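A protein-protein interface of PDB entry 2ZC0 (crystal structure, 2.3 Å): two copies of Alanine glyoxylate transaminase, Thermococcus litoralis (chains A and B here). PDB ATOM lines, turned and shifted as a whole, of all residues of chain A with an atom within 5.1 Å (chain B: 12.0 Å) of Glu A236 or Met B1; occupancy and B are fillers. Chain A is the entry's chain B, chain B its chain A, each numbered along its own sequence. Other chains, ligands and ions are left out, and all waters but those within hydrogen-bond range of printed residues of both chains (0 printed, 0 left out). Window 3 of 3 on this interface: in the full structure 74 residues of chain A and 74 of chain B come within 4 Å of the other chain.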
ATOM      1  N   SER A 205      17.048   4.132  27.787  1.00  0.00           N
ATOM      2  CA  SER A 205      15.671   4.504  28.085  1.00  0.00           C
ATOM      3  C   SER A 205      15.602   5.908  28.683  1.00  0.00           C
ATOM      4  O   SER A 205      14.759   6.731  28.284  1.00  0.00           O
ATOM      5  CB  SER A 205      15.068   3.483  29.051  1.00  0.00           C
ATOM      6  OG  SER A 205      13.768   3.853  29.466  1.00  0.00           O
ATOM      7  N   ASP A 234      15.813  -6.388  25.998  1.00  0.00           N
ATOM      8  CA  ASP A 234      15.177  -5.210  25.395  1.00  0.00           C
ATOM      9  C   ASP A 234      13.643  -5.210  25.457  1.00  0.00           C
ATOM     10  O   ASP A 234      12.966  -5.547  24.477  1.00  0.00           O
ATOM     11  CB  ASP A 234      15.647  -5.119  23.931  1.00  0.00           C
ATOM     12  CG  ASP A 234      15.192  -3.857  23.233  1.00  0.00           C
ATOM     13  OD1 ASP A 234      14.948  -3.927  22.015  1.00  0.00           O
ATOM     14  OD2 ASP A 234      15.096  -2.797  23.882  1.00  0.00           O
ATOM     15  N   ASN A 235      13.094  -4.820  26.601  1.00  0.00           N
ATOM     16  CA  ASN A 235      11.650  -4.794  26.768  1.00  0.00           C
ATOM     17  C   ASN A 235      11.020  -3.543  26.149  1.00  0.00           C
ATOM     18  O   ASN A 235       9.818  -3.527  25.873  1.00  0.00           O
ATOM     19  CB  ASN A 235      11.300  -4.864  28.253  1.00  0.00           C
ATOM     20  CG  ASN A 235      11.738  -3.630  29.002  1.00  0.00           C
ATOM     21  OD1 ASN A 235      12.928  -3.285  29.015  1.00  0.00           O
ATOM     22  ND2 ASN A 235      10.780  -2.945  29.627  1.00  0.00           N
ATOM     23  N   GLU A 236      11.824  -2.500  25.934  1.00  0.00           N
ATOM     24  CA  GLU A 236      11.329  -1.259  25.329  1.00  0.00           C
ATOM     25  C   GLU A 236      11.557  -1.193  23.822  1.00  0.00           C
ATOM     26  O   GLU A 236      11.204  -0.205  23.188  1.00  0.00           O
ATOM     27  CB  GLU A 236      11.980  -0.028  25.984  1.00  0.00           C
ATOM     28  CG  GLU A 236      11.601   0.164  27.449  1.00  0.00           C
ATOM     29  CD  GLU A 236      12.100   1.470  28.052  1.00  0.00           C
ATOM     30  OE1 GLU A 236      11.697   1.759  29.195  1.00  0.00           O
ATOM     31  OE2 GLU A 236      12.884   2.206  27.412  1.00  0.00           O
ATOM     32  N   GLY A 237      12.148  -2.237  23.253  1.00  0.00           N
ATOM     33  CA  GLY A 237      12.403  -2.256  21.819  1.00  0.00           C
ATOM     34  C   GLY A 237      13.405  -1.219  21.319  1.00  0.00           C
ATOM     35  O   GLY A 237      13.293  -0.738  20.192  1.00  0.00           O
ATOM     36  N   ARG A 238      14.384  -0.871  22.159  1.00  0.00           N
ATOM     37  CA  ARG A 238      15.412   0.115  21.802  1.00  0.00           C
ATOM     38  C   ARG A 238      16.672  -0.493  21.217  1.00  0.00           C
ATOM     39  O   ARG A 238      17.607   0.238  20.915  1.00  0.00           O
ATOM     40  CB  ARG A 238      15.813   0.956  23.014  1.00  0.00           C
ATOM     41  CG  ARG A 238      14.755   1.928  23.488  1.00  0.00           C
ATOM     42  CD  ARG A 238      15.152   2.660  24.785  1.00  0.00           C
ATOM     43  NE  ARG A 238      14.156   3.667  25.119  1.00  0.00           N
ATOM     44  CZ  ARG A 238      13.938   4.761  24.397  1.00  0.00           C
ATOM     45  NH1 ARG A 238      13.000   5.630  24.761  1.00  0.00           N
ATOM     46  NH2 ARG A 238      14.678   5.002  23.323  1.00  0.00           N
ATOM     47  N   GLU A 263       9.035   0.965  11.696  1.00  0.00           N
ATOM     48  CA  GLU A 263       9.489   1.741  10.551  1.00  0.00           C
ATOM     49  C   GLU A 263      10.964   1.568  10.184  1.00  0.00           C
ATOM     50  O   GLU A 263      11.333   1.727   9.016  1.00  0.00           O
ATOM     51  CB  GLU A 263       9.189   3.219  10.787  1.00  0.00           C
ATOM     52  CG  GLU A 263       7.704   3.552  10.938  1.00  0.00           C
ATOM     53  CD  GLU A 263       7.088   3.018  12.222  1.00  0.00           C
ATOM     54  OE1 GLU A 263       7.813   2.876  13.236  1.00  0.00           O
ATOM     55  OE2 GLU A 263       5.868   2.755  12.223  1.00  0.00           O
ATOM     56  N   MET B   1       5.901   1.780  20.037  1.00  0.00           N
ATOM     57  CA  MET B   1       6.931   2.855  19.929  1.00  0.00           C
ATOM     58  C   MET B   1       6.992   3.354  18.489  1.00  0.00           C
ATOM     59  O   MET B   1       6.798   2.580  17.548  1.00  0.00           O
ATOM     60  CB  MET B   1       8.311   2.324  20.351  1.00  0.00           C
ATOM     61  CG  MET B   1       9.363   3.417  20.467  1.00  0.00           C
ATOM     62  SD  MET B   1      10.976   2.908  21.123  1.00  0.00           S
ATOM     63  CE  MET B   1      10.646   2.928  22.889  1.00  0.00           C
ATOM     64  N   ASP B   2       7.260   4.647  18.318  1.00  0.00           N
ATOM     65  CA  ASP B   2       7.341   5.259  16.990  1.00  0.00           C
ATOM     66  C   ASP B   2       8.808   5.353  16.556  1.00  0.00           C
ATOM     67  O   ASP B   2       9.501   6.299  16.914  1.00  0.00           O
ATOM     68  CB  ASP B   2       6.714   6.658  17.036  1.00  0.00           C
ATOM     69  CG  ASP B   2       6.698   7.352  15.677  1.00  0.00           C
ATOM     70  OD1 ASP B   2       6.396   8.565  15.643  1.00  0.00           O
ATOM     71  OD2 ASP B   2       6.974   6.698  14.648  1.00  0.00           O
ATOM     72  N   TYR B   3       9.282   4.380  15.784  1.00  0.00           N
ATOM     73  CA  TYR B   3      10.682   4.402  15.356  1.00  0.00           C
ATOM     74  C   TYR B   3      10.942   5.429  14.283  1.00  0.00           C
ATOM     75  O   TYR B   3      12.090   5.711  13.949  1.00  0.00           O
ATOM     76  CB  TYR B   3      11.114   3.033  14.849  1.00  0.00           C
ATOM     77  CG  TYR B   3      11.105   1.981  15.923  1.00  0.00           C
ATOM     78  CD1 TYR B   3       9.998   1.149  16.102  1.00  0.00           C
ATOM     79  CD2 TYR B   3      12.191   1.838  16.786  1.00  0.00           C
ATOM     80  CE1 TYR B   3       9.975   0.198  17.120  1.00  0.00           C
ATOM     81  CE2 TYR B   3      12.174   0.893  17.806  1.00  0.00           C
ATOM     82  CZ  TYR B   3      11.068   0.078  17.966  1.00  0.00           C
ATOM     83  OH  TYR B   3      11.063  -0.853  18.969  1.00  0.00           O
ATOM     84  N   THR B   4       9.867   5.989  13.746  1.00  0.00           N
ATOM     85  CA  THR B   4       9.986   6.980  12.693  1.00  0.00           C
ATOM     86  C   THR B   4      10.836   8.182  13.134  1.00  0.00           C
ATOM     87  O   THR B   4      11.623   8.711  12.349  1.00  0.00           O
ATOM     88  CB  THR B   4       8.579   7.422  12.224  1.00  0.00           C
ATOM     89  OG1 THR B   4       8.619   7.719  10.834  1.00  0.00           O
ATOM     90  CG2 THR B   4       8.105   8.635  12.982  1.00  0.00           C
ATOM     91  N   LYS B   5      10.709   8.577  14.398  1.00  0.00           N
ATOM     92  CA  LYS B   5      11.446   9.718  14.948  1.00  0.00           C
ATOM     93  C   LYS B   5      12.961   9.522  15.004  1.00  0.00           C
ATOM     94  O   LYS B   5      13.717  10.493  15.117  1.00  0.00           O
ATOM     95  CB  LYS B   5      10.936  10.047  16.358  1.00  0.00           C
ATOM     96  CG  LYS B   5       9.416   9.989  16.504  1.00  0.00           C
ATOM     97  CD  LYS B   5       8.945  10.492  17.876  1.00  0.00           C
ATOM     98  CE  LYS B   5       8.876  12.030  17.953  1.00  0.00           C
ATOM     99  NZ  LYS B   5      10.173  12.765  17.739  1.00  0.00           N
ATOM    100  N   TYR B   6      13.411   8.275  14.929  1.00  0.00           N
ATOM    101  CA  TYR B   6      14.842   8.004  14.976  1.00  0.00           C
ATOM    102  C   TYR B   6      15.458   7.903  13.585  1.00  0.00           C
ATOM    103  O   TYR B   6      16.685   7.869  13.444  1.00  0.00           O
ATOM    104  CB  TYR B   6      15.108   6.717  15.772  1.00  0.00           C
ATOM    105  CG  TYR B   6      14.385   6.693  17.106  1.00  0.00           C
ATOM    106  CD1 TYR B   6      13.047   6.300  17.183  1.00  0.00           C
ATOM    107  CD2 TYR B   6      15.020   7.116  18.283  1.00  0.00           C
ATOM    108  CE1 TYR B   6      12.351   6.329  18.390  1.00  0.00           C
ATOM    109  CE2 TYR B   6      14.328   7.147  19.501  1.00  0.00           C
ATOM    110  CZ  TYR B   6      12.993   6.751  19.540  1.00  0.00           C
ATOM    111  OH  TYR B   6      12.281   6.767  20.715  1.00  0.00           O
ATOM    112  N   LEU B   7      14.615   7.869  12.556  1.00  0.00           N
ATOM    113  CA  LEU B   7      15.107   7.760  11.181  1.00  0.00           C
ATOM    114  C   LEU B   7      15.978   8.936  10.767  1.00  0.00           C
ATOM    115  O   LEU B   7      15.875  10.026  11.322  1.00  0.00           O
ATOM    116  CB  LEU B   7      13.932   7.650  10.191  1.00  0.00           C
ATOM    117  CG  LEU B   7      13.094   6.373  10.199  1.00  0.00           C
ATOM    118  CD1 LEU B   7      11.891   6.579   9.313  1.00  0.00           C
ATOM    119  CD2 LEU B   7      13.907   5.188   9.721  1.00  0.00           C
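The side-chain hydroxyl (OH) of Tyr B3 is in hydrogen-bond range of the backbone carbonyl oxygen (O) of Gly A237. N of Tyr B3 sits at hydrogen-bond distance from OE1 of Glu A263. The backbone carbonyl oxygen (O) of Glu A236 lies close to the side-chain sulfur (SD) of Met B1, 3.7 Å away.
The side-chain carboxylate (OD2) of Asp B2 sits close to the backbone NH (N) of Thr B4 (3.1 Å). The side-chain carboxylate (OE2) of Glu A236 sits at hydrogen-bond distance from the side-chain hydroxyl (OG) of Ser A205. The side-chain carboxylate (OD2) of Asp A234 lies within hydrogen-bond range of the backbone NH (N) of Gly A237. The side-chain carboxylate of Asp A234 is in hydrogen-bond range of the backbone NH of Arg A238 (2.7 Å). The side-chain carboxylate of Glu A236 lies within salt-bridge range of the guanidinium group of Arg A238.
Among the printed residues, merely in contact across the chains: Arg A238 with Tyr B6 (3.96 Å) and Glu A263 with Thr B4 (3.8 Å).
Of chain B, only Met B1 comes within 4 Å of Glu A236. Met B1 touches one residue of chain A. No residue of chain B comes within 4 Å of Asp A234. No residue of chain B comes within 4 Å of Asn A235. Arg A238 touches just one residue of chain B: Tyr B6. Printed residues of chain A within 4 Å of Tyr B3: Gly A237 and Glu A263. Printed residues of chain B within 4 Å of Glu A263: Tyr B3 and Thr B4. Printed residues of chain A within 4 Å of Tyr B6: Arg A238 (3.96 Å). Printed residues of chain A within 4 Å of Thr B4: Glu A263. Lys B5 touches none of the printed residues of chain A. The nearest printed residue of chain A that does not touch Tyr B6 is Gly A237 (7.4 Å).
Of the 7 printed residues of chain A, 4 touch a printed residue of chain B. Hydrophobic or aromatic side chains of chain B within 4 Å of the printed part of chain A: Met B1, Tyr B3 and Tyr B6. Among the printed residues, no Asp or Glu carboxylate lies within 4 Å of a Lys or Arg side-chain nitrogen of the other chain.
No position is printed for both chains. Of the 5 pairs that touch across the chains among the printed residues, none has its exchanged pair printed and touching as well.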
